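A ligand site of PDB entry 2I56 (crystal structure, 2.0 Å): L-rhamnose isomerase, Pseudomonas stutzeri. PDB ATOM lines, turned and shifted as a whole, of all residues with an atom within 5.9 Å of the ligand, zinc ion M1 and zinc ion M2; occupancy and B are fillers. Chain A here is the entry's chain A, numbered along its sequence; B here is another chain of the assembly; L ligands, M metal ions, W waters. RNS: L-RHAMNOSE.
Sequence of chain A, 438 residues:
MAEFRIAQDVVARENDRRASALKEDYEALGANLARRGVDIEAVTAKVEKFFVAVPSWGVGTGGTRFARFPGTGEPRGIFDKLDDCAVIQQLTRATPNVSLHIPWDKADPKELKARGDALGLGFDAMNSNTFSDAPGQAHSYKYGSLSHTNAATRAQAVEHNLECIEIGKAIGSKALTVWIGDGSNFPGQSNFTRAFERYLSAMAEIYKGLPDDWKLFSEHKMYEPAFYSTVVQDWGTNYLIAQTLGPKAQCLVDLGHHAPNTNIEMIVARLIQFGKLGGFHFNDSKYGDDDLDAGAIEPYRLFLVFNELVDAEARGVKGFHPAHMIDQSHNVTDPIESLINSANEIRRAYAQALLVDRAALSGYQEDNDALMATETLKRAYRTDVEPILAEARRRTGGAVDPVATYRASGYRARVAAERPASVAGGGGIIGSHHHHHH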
ATOM      1  N   TRP A  57       6.250  10.178   3.587  1.00  0.00           N
ATOM      2  CA  TRP A  57       5.792   9.042   4.386  1.00  0.00           C
ATOM      3  C   TRP A  57       6.898   8.198   5.031  1.00  0.00           C
ATOM      4  O   TRP A  57       6.614   7.280   5.805  1.00  0.00           O
ATOM      5  CB  TRP A  57       4.868   8.138   3.538  1.00  0.00           C
ATOM      6  CG  TRP A  57       5.506   7.523   2.332  1.00  0.00           C
ATOM      7  CD1 TRP A  57       6.109   6.304   2.242  1.00  0.00           C
ATOM      8  CD2 TRP A  57       5.595   8.099   1.021  1.00  0.00           C
ATOM      9  NE1 TRP A  57       6.560   6.075   0.971  1.00  0.00           N
ATOM     10  CE2 TRP A  57       6.262   7.165   0.195  1.00  0.00           C
ATOM     11  CE3 TRP A  57       5.168   9.314   0.468  1.00  0.00           C
ATOM     12  CZ2 TRP A  57       6.506   7.411  -1.163  1.00  0.00           C
ATOM     13  CZ3 TRP A  57       5.419   9.555  -0.885  1.00  0.00           C
ATOM     14  CH2 TRP A  57       6.087   8.614  -1.674  1.00  0.00           C
ATOM     15  N   HIS A 101       2.096  12.619  -0.366  1.00  0.00           N
ATOM     16  CA  HIS A 101       1.139  11.535  -0.546  1.00  0.00           C
ATOM     17  C   HIS A 101      -0.229  12.035  -0.071  1.00  0.00           C
ATOM     18  O   HIS A 101      -0.354  12.558   1.028  1.00  0.00           O
ATOM     19  CB  HIS A 101       1.578  10.319   0.281  1.00  0.00           C
ATOM     20  CG  HIS A 101       1.336   9.018  -0.402  1.00  0.00           C
ATOM     21  ND1 HIS A 101       0.076   8.592  -0.774  1.00  0.00           N
ATOM     22  CD2 HIS A 101       2.192   8.038  -0.782  1.00  0.00           C
ATOM     23  CE1 HIS A 101       0.174   7.407  -1.356  1.00  0.00           C
ATOM     24  NE2 HIS A 101       1.440   7.051  -1.382  1.00  0.00           N
ATOM     25  N   TRP A 104      -2.854  11.524   2.966  1.00  0.00           N
ATOM     26  CA  TRP A 104      -2.055  11.659   4.195  1.00  0.00           C
ATOM     27  C   TRP A 104      -1.551  13.075   4.429  1.00  0.00           C
ATOM     28  O   TRP A 104      -1.642  13.608   5.529  1.00  0.00           O
ATOM     29  CB  TRP A 104      -0.843  10.722   4.191  1.00  0.00           C
ATOM     30  CG  TRP A 104      -1.164   9.255   4.158  1.00  0.00           C
ATOM     31  CD1 TRP A 104      -2.315   8.658   4.563  1.00  0.00           C
ATOM     32  CD2 TRP A 104      -0.302   8.209   3.692  1.00  0.00           C
ATOM     33  NE1 TRP A 104      -2.227   7.297   4.389  1.00  0.00           N
ATOM     34  CE2 TRP A 104      -1.001   6.989   3.850  1.00  0.00           C
ATOM     35  CE3 TRP A 104       0.994   8.175   3.165  1.00  0.00           C
ATOM     36  CZ2 TRP A 104      -0.455   5.755   3.501  1.00  0.00           C
ATOM     37  CZ3 TRP A 104       1.546   6.944   2.808  1.00  0.00           C
ATOM     38  CH2 TRP A 104       0.819   5.751   2.977  1.00  0.00           C
ATOM     39  N   ASN A 127       1.788  11.654  -5.134  1.00  0.00           N
ATOM     40  CA  ASN A 127       1.485  10.231  -5.081  1.00  0.00           C
ATOM     41  C   ASN A 127       0.027  10.064  -4.668  1.00  0.00           C
ATOM     42  O   ASN A 127      -0.390  10.604  -3.644  1.00  0.00           O
ATOM     43  CB  ASN A 127       2.381   9.533  -4.053  1.00  0.00           C
ATOM     44  CG  ASN A 127       3.849   9.548  -4.453  1.00  0.00           C
ATOM     45  OD1 ASN A 127       4.333   8.632  -5.107  1.00  0.00           O
ATOM     46  ND2 ASN A 127       4.552  10.606  -4.077  1.00  0.00           N
ATOM     47  N   SER A 128      -0.744   9.320  -5.456  1.00  0.00           N
ATOM     48  CA  SER A 128      -2.145   9.103  -5.126  1.00  0.00           C
ATOM     49  C   SER A 128      -2.298   7.887  -4.208  1.00  0.00           C
ATOM     50  O   SER A 128      -1.395   7.054  -4.115  1.00  0.00           O
ATOM     51  CB  SER A 128      -2.977   8.906  -6.394  1.00  0.00           C
ATOM     52  OG  SER A 128      -2.480   7.830  -7.162  1.00  0.00           O
ATOM     53  N   PHE A 131      -5.222   2.601  -2.365  1.00  0.00           N
ATOM     54  CA  PHE A 131      -4.891   1.273  -1.846  1.00  0.00           C
ATOM     55  C   PHE A 131      -5.370   1.162  -0.392  1.00  0.00           C
ATOM     56  O   PHE A 131      -5.089   0.177   0.305  1.00  0.00           O
ATOM     57  CB  PHE A 131      -3.384   0.992  -1.967  1.00  0.00           C
ATOM     58  CG  PHE A 131      -2.494   2.038  -1.353  1.00  0.00           C
ATOM     59  CD1 PHE A 131      -2.354   2.144   0.026  1.00  0.00           C
ATOM     60  CD2 PHE A 131      -1.780   2.922  -2.170  1.00  0.00           C
ATOM     61  CE1 PHE A 131      -1.514   3.107   0.584  1.00  0.00           C
ATOM     62  CE2 PHE A 131      -0.934   3.886  -1.620  1.00  0.00           C
ATOM     63  CZ  PHE A 131      -0.803   3.982  -0.237  1.00  0.00           C
ATOM     64  N   THR A 177       2.627  10.085  -9.488  1.00  0.00           N
ATOM     65  CA  THR A 177       3.016   8.681  -9.449  1.00  0.00           C
ATOM     66  C   THR A 177       1.812   7.882  -9.001  1.00  0.00           C
ATOM     67  O   THR A 177       1.179   8.206  -7.995  1.00  0.00           O
ATOM     68  CB  THR A 177       4.152   8.437  -8.446  1.00  0.00           C
ATOM     69  OG1 THR A 177       5.330   9.108  -8.903  1.00  0.00           O
ATOM     70  CG2 THR A 177       4.421   6.936  -8.314  1.00  0.00           C
ATOM     71  N   TRP A 179       0.654   4.163  -7.842  1.00  0.00           N
ATOM     72  CA  TRP A 179       0.887   2.795  -7.429  1.00  0.00           C
ATOM     73  C   TRP A 179      -0.400   2.359  -6.748  1.00  0.00           C
ATOM     74  O   TRP A 179      -0.898   3.058  -5.861  1.00  0.00           O
ATOM     75  CB  TRP A 179       2.017   2.661  -6.406  1.00  0.00           C
ATOM     76  CG  TRP A 179       2.097   1.246  -5.902  1.00  0.00           C
ATOM     77  CD1 TRP A 179       2.525   0.149  -6.600  1.00  0.00           C
ATOM     78  CD2 TRP A 179       1.598   0.748  -4.650  1.00  0.00           C
ATOM     79  NE1 TRP A 179       2.310  -1.000  -5.864  1.00  0.00           N
ATOM     80  CE2 TRP A 179       1.748  -0.659  -4.662  1.00  0.00           C
ATOM     81  CE3 TRP A 179       1.039   1.357  -3.514  1.00  0.00           C
ATOM     82  CZ2 TRP A 179       1.350  -1.468  -3.595  1.00  0.00           C
ATOM     83  CZ3 TRP A 179       0.638   0.538  -2.450  1.00  0.00           C
ATOM     84  CH2 TRP A 179       0.796  -0.851  -2.503  1.00  0.00           C
ATOM     85  N   GLU A 219       3.727   2.598 -11.475  1.00  0.00           N
ATOM     86  CA  GLU A 219       4.699   1.765 -10.775  1.00  0.00           C
ATOM     87  C   GLU A 219       4.278   0.305 -10.653  1.00  0.00           C
ATOM     88  O   GLU A 219       3.231   0.003 -10.067  1.00  0.00           O
ATOM     89  CB  GLU A 219       4.934   2.353  -9.370  1.00  0.00           C
ATOM     90  CG  GLU A 219       5.828   1.528  -8.461  1.00  0.00           C
ATOM     91  CD  GLU A 219       6.108   2.233  -7.135  1.00  0.00           C
ATOM     92  OE1 GLU A 219       5.369   3.176  -6.791  1.00  0.00           O
ATOM     93  OE2 GLU A 219       7.061   1.840  -6.427  1.00  0.00           O
ATOM     94  N   LYS A 221       4.618  -3.764  -9.496  1.00  0.00           N
ATOM     95  CA  LYS A 221       4.969  -4.490  -8.285  1.00  0.00           C
ATOM     96  C   LYS A 221       4.487  -5.928  -8.444  1.00  0.00           C
ATOM     97  O   LYS A 221       3.320  -6.161  -8.754  1.00  0.00           O
ATOM     98  CB  LYS A 221       4.322  -3.849  -7.054  1.00  0.00           C
ATOM     99  CG  LYS A 221       4.851  -4.407  -5.723  1.00  0.00           C
ATOM    100  CD  LYS A 221       4.209  -3.720  -4.517  1.00  0.00           C
ATOM    101  CE  LYS A 221       4.780  -4.272  -3.205  1.00  0.00           C
ATOM    102  NZ  LYS A 221       4.151  -3.648  -2.002  1.00  0.00           N
ATOM    103  N   GLU A 224       1.868  -8.072  -3.211  1.00  0.00           N
ATOM    104  CA  GLU A 224       1.657  -7.315  -1.973  1.00  0.00           C
ATOM    105  C   GLU A 224       1.138  -5.918  -2.300  1.00  0.00           C
ATOM    106  O   GLU A 224       1.857  -5.104  -2.863  1.00  0.00           O
ATOM    107  CB  GLU A 224       2.927  -7.161  -1.110  1.00  0.00           C
ATOM    108  CG  GLU A 224       2.622  -6.404   0.197  1.00  0.00           C
ATOM    109  CD  GLU A 224       3.838  -5.847   0.906  1.00  0.00           C
ATOM    110  OE1 GLU A 224       4.785  -5.392   0.230  1.00  0.00           O
ATOM    111  OE2 GLU A 224       3.836  -5.847   2.157  1.00  0.00           O
ATOM    112  N   LEU A 252       7.949   3.737 -13.618  1.00  0.00           N
ATOM    113  CA  LEU A 252       8.774   3.968 -12.436  1.00  0.00           C
ATOM    114  C   LEU A 252       9.234   2.615 -11.915  1.00  0.00           C
ATOM    115  O   LEU A 252       8.428   1.694 -11.757  1.00  0.00           O
ATOM    116  CB  LEU A 252       7.957   4.732 -11.392  1.00  0.00           C
ATOM    117  CG  LEU A 252       8.714   5.209 -10.156  1.00  0.00           C
ATOM    118  CD1 LEU A 252       8.210   6.590  -9.756  1.00  0.00           C
ATOM    119  CD2 LEU A 252       8.557   4.187  -9.033  1.00  0.00           C
ATOM    120  N   ASP A 254      10.747   0.565  -8.884  1.00  0.00           N
ATOM    121  CA  ASP A 254      11.016   0.527  -7.454  1.00  0.00           C
ATOM    122  C   ASP A 254      11.839  -0.738  -7.264  1.00  0.00           C
ATOM    123  O   ASP A 254      11.359  -1.850  -7.488  1.00  0.00           O
ATOM    124  CB  ASP A 254       9.713   0.451  -6.654  1.00  0.00           C
ATOM    125  CG  ASP A 254       9.954   0.471  -5.156  1.00  0.00           C
ATOM    126  OD1 ASP A 254       9.289   1.264  -4.449  1.00  0.00           O
ATOM    127  OD2 ASP A 254      10.798  -0.309  -4.678  1.00  0.00           O
ATOM    128  N   HIS A 257      10.552  -4.208  -5.967  1.00  0.00           N
ATOM    129  CA  HIS A 257       9.314  -4.733  -6.534  1.00  0.00           C
ATOM    130  C   HIS A 257       9.432  -5.836  -7.577  1.00  0.00           C
ATOM    131  O   HIS A 257       8.482  -6.079  -8.335  1.00  0.00           O
ATOM    132  CB  HIS A 257       8.500  -3.589  -7.149  1.00  0.00           C
ATOM    133  CG  HIS A 257       7.945  -2.632  -6.146  1.00  0.00           C
ATOM    134  ND1 HIS A 257       6.951  -1.727  -6.455  1.00  0.00           N
ATOM    135  CD2 HIS A 257       8.221  -2.447  -4.838  1.00  0.00           C
ATOM    136  CE1 HIS A 257       6.647  -1.016  -5.384  1.00  0.00           C
ATOM    137  NE2 HIS A 257       7.414  -1.436  -4.390  1.00  0.00           N
ATOM    138  N   HIS A 281      12.462   4.485  -7.514  1.00  0.00           N
ATOM    139  CA  HIS A 281      12.074   4.476  -6.121  1.00  0.00           C
ATOM    140  C   HIS A 281      13.207   3.648  -5.528  1.00  0.00           C
ATOM    141  O   HIS A 281      13.226   2.421  -5.660  1.00  0.00           O
ATOM    142  CB  HIS A 281      10.733   3.779  -5.892  1.00  0.00           C
ATOM    143  CG  HIS A 281       9.574   4.727  -5.807  1.00  0.00           C
ATOM    144  ND1 HIS A 281       8.332   4.347  -5.320  1.00  0.00           N
ATOM    145  CD2 HIS A 281       9.459   6.036  -6.145  1.00  0.00           C
ATOM    146  CE1 HIS A 281       7.511   5.377  -5.371  1.00  0.00           C
ATOM    147  NE2 HIS A 281       8.162   6.415  -5.859  1.00  0.00           N
ATOM    148  N   ASN A 283      15.637   1.930  -2.717  1.00  0.00           N
ATOM    149  CA  ASN A 283      15.563   1.217  -1.451  1.00  0.00           C
ATOM    150  C   ASN A 283      16.377  -0.056  -1.662  1.00  0.00           C
ATOM    151  O   ASN A 283      16.956  -0.257  -2.732  1.00  0.00           O
ATOM    152  CB  ASN A 283      14.116   0.853  -1.075  1.00  0.00           C
ATOM    153  CG  ASN A 283      13.327   0.233  -2.215  1.00  0.00           C
ATOM    154  OD1 ASN A 283      13.753  -0.752  -2.827  1.00  0.00           O
ATOM    155  ND2 ASN A 283      12.169   0.812  -2.502  1.00  0.00           N
ATOM    156  N   ASP A 289       9.569  -6.942  -0.969  1.00  0.00           N
ATOM    157  CA  ASP A 289       9.580  -5.478  -1.027  1.00  0.00           C
ATOM    158  C   ASP A 289       9.879  -5.017   0.397  1.00  0.00           C
ATOM    159  O   ASP A 289       9.037  -4.407   1.059  1.00  0.00           O
ATOM    160  CB  ASP A 289       8.223  -4.956  -1.499  1.00  0.00           C
ATOM    161  CG  ASP A 289       8.156  -3.442  -1.504  1.00  0.00           C
ATOM    162  OD1 ASP A 289       9.191  -2.791  -1.743  1.00  0.00           O
ATOM    163  OD2 ASP A 289       7.046  -2.900  -1.283  1.00  0.00           O
ATOM    164  N   ASP A 291      11.747  -2.660   1.547  1.00  0.00           N
ATOM    165  CA  ASP A 291      11.861  -1.213   1.751  1.00  0.00           C
ATOM    166  C   ASP A 291      12.957  -0.794   2.732  1.00  0.00           C
ATOM    167  O   ASP A 291      12.766   0.134   3.518  1.00  0.00           O
ATOM    168  CB  ASP A 291      10.518  -0.638   2.199  1.00  0.00           C
ATOM    169  CG  ASP A 291       9.463  -0.711   1.109  1.00  0.00           C
ATOM    170  OD1 ASP A 291       9.846  -0.582  -0.071  1.00  0.00           O
ATOM    171  OD2 ASP A 291       8.264  -0.872   1.411  1.00  0.00           O
ATOM    172  N   ASP A 327      12.002   5.495  -1.623  1.00  0.00           N
ATOM    173  CA  ASP A 327      10.748   4.964  -1.129  1.00  0.00           C
ATOM    174  C   ASP A 327      11.120   3.862  -0.149  1.00  0.00           C
ATOM    175  O   ASP A 327      11.353   2.722  -0.545  1.00  0.00           O
ATOM    176  CB  ASP A 327       9.881   4.379  -2.255  1.00  0.00           C
ATOM    177  CG  ASP A 327       8.546   3.851  -1.756  1.00  0.00           C
ATOM    178  OD1 ASP A 327       8.283   3.953  -0.538  1.00  0.00           O
ATOM    179  OD2 ASP A 327       7.750   3.344  -2.573  1.00  0.00           O
ATOM    180  N   ARG B  65       0.166  -4.385   5.501  1.00  0.00           N
ATOM    181  CA  ARG B  65       0.712  -3.167   6.076  1.00  0.00           C
ATOM    182  C   ARG B  65       0.153  -1.921   5.395  1.00  0.00           C
ATOM    183  O   ARG B  65       0.371  -0.800   5.868  1.00  0.00           O
ATOM    184  CB  ARG B  65       2.239  -3.152   5.984  1.00  0.00           C
ATOM    185  CG  ARG B  65       2.765  -3.196   4.569  1.00  0.00           C
ATOM    186  CD  ARG B  65       4.277  -3.007   4.543  1.00  0.00           C
ATOM    187  NE  ARG B  65       4.834  -3.396   3.252  1.00  0.00           N
ATOM    188  CZ  ARG B  65       5.882  -2.797   2.682  1.00  0.00           C
ATOM    189  NH1 ARG B  65       6.485  -1.782   3.291  1.00  0.00           N
ATOM    190  NH2 ARG B  65       6.297  -3.207   1.495  1.00  0.00           N
ATOM    191  N   PHE B  66      -0.549  -2.090   4.280  1.00  0.00           N
ATOM    192  CA  PHE B  66      -1.120  -0.952   3.566  1.00  0.00           C
ATOM    193  C   PHE B  66      -2.562  -0.684   3.947  1.00  0.00           C
ATOM    194  O   PHE B  66      -3.012   0.456   3.892  1.00  0.00           O
ATOM    195  CB  PHE B  66      -1.039  -1.183   2.057  1.00  0.00           C
ATOM    196  CG  PHE B  66       0.368  -1.263   1.540  1.00  0.00           C
ATOM    197  CD1 PHE B  66       1.127  -0.113   1.359  1.00  0.00           C
ATOM    198  CD2 PHE B  66       0.948  -2.499   1.265  1.00  0.00           C
ATOM    199  CE1 PHE B  66       2.442  -0.184   0.915  1.00  0.00           C
ATOM    200  CE2 PHE B  66       2.262  -2.586   0.829  1.00  0.00           C
ATOM    201  CZ  PHE B  66       3.017  -1.422   0.648  1.00  0.00           C
HETATM  202  C1  RNS L   1       4.252   0.152  -2.575  1.00  0.00           C
HETATM  203  C2  RNS L   1       4.940   1.153  -3.487  1.00  0.00           C
HETATM  204  C3  RNS L   1       4.332   2.549  -3.324  1.00  0.00           C
HETATM  205  C4  RNS L   1       4.139   2.907  -1.844  1.00  0.00           C
HETATM  206  C5  RNS L   1       3.802   4.390  -1.701  1.00  0.00           C
HETATM  207  C6  RNS L   1       3.521   4.705  -0.234  1.00  0.00           C
HETATM  208  O1  RNS L   1       4.781  -0.938  -2.349  1.00  0.00           O
HETATM  209  O2  RNS L   1       6.329   1.203  -3.192  1.00  0.00           O
HETATM  210  O3  RNS L   1       5.173   3.505  -3.955  1.00  0.00           O
HETATM  211  O4  RNS L   1       5.320   2.615  -1.109  1.00  0.00           O
HETATM  212  O5  RNS L   1       2.669   4.711  -2.483  1.00  0.00           O
HETATM  213 ZN    ZN M   1       7.579   2.650  -4.523  1.00  0.00          ZN
HETATM  214 ZN    ZN M   2       6.938  -0.990  -2.355  1.00  0.00          ZN
HETATM  215  O   HOH W   1       8.688   0.019  -2.149  1.00  0.00           O
HETATM  216  O   HOH W   2       3.117   5.968  -4.717  1.00  0.00           O
HETATM  217  O   HOH W   3       6.113   0.053  -0.143  1.00  0.00           O
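NE2 of His 101 is in hydrogen-bond range of O5 of the ligand, at 2.9 Å. The side-chain amino group (NZ) of Lys 221 sits close to an oxygen (O1) of the ligand (2.8 Å).
O of Asp 289 is in hydrogen-bond range of NH2 of Arg 65 of chain B (3.0 Å). NE1 of Trp 57 is in hydrogen-bond range of OD1 of Asp 327 (3.1 Å). OD2 of Asp 291 is in salt-bridge range of NH1 of Arg 65 of chain B (2.7 Å). OD2 of Asp 289 sits close to NZ of Lys 221, 3.1 Å away. The side-chain amino group (NZ) of Lys 221 is in salt-bridge range of the side-chain carboxylate (OE1) of Glu 224 (2.9 Å). The backbone carbonyl oxygen (O) of Asp 327 lies within hydrogen-bond range of the side-chain amide nitrogen (ND2) of Asn 283. The side-chain carboxylate of Asp 254 lies within hydrogen-bond range of the side-chain amide nitrogen of Asn 283 (2.8 Å).
Trp 57 touches the ligand (NE1 to C6, 3.5 Å). Phe 131 touches the ligand (CE2 to O5, 3.8 Å). Trp 179 touches the ligand (CE2 to C1, 3.4 Å). CZ of Phe 66 of chain B touches O1 of the ligand (3.5 Å). Hydrophobic or aromatic side chains within 4 Å of the ligand: Trp 57, His 101, Phe 131, Trp 179, His 257, His 281 and Phe 66 of chain B. 12 residues have an atom within 4 Å of the ligand: Trp 57, His 101, Phe 131, Trp 179, Glu 219, Lys 221, Asp 254, His 257, His 281, Asp 289, Asp 327 and Phe 66 of chain B. The nearest printed residue that does not touch the ligand is Trp 104 (4.3 Å).
Residues that only touch zinc ion M2: Lys 221 (3.9 Å) and Asp 291 (3.7 Å).
Zinc ion M1 is bound by a ring nitrogen (ND1) of His 281 (2.0 Å), the side-chain carboxylate (OD2) of Asp 327 (2.1 Å), the side-chain carboxylate (OE2) of Glu 219 (2.1 Å), the side-chain carboxylate (OD1) of Asp 254 (2.2 Å) and an oxygen (O2) of the ligand (2.3 Å). Slightly farther from zinc ion M1 lies an oxygen (O3) of the ligand (2.6 Å).
Zinc ion M2 is bound by water W1 (2.0 Å), NE2 of His 257 (2.1 Å), O1 of the ligand (2.2 Å), OD2 of Asp 289 (2.2 Å), O2 of the ligand (2.4 Å) and water W3 (2.6 Å). Zinc ion M2 has six donor atoms within binding distance.
Water W3 bridges the side-chain carboxylate of Asp 291 and an oxygen (O4) of the ligand. Water W2 lies within hydrogen-bond range of an oxygen (O5) of the ligand (2.6 Å) and the side-chain amide oxygen of Asn 127 (3.0 Å).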
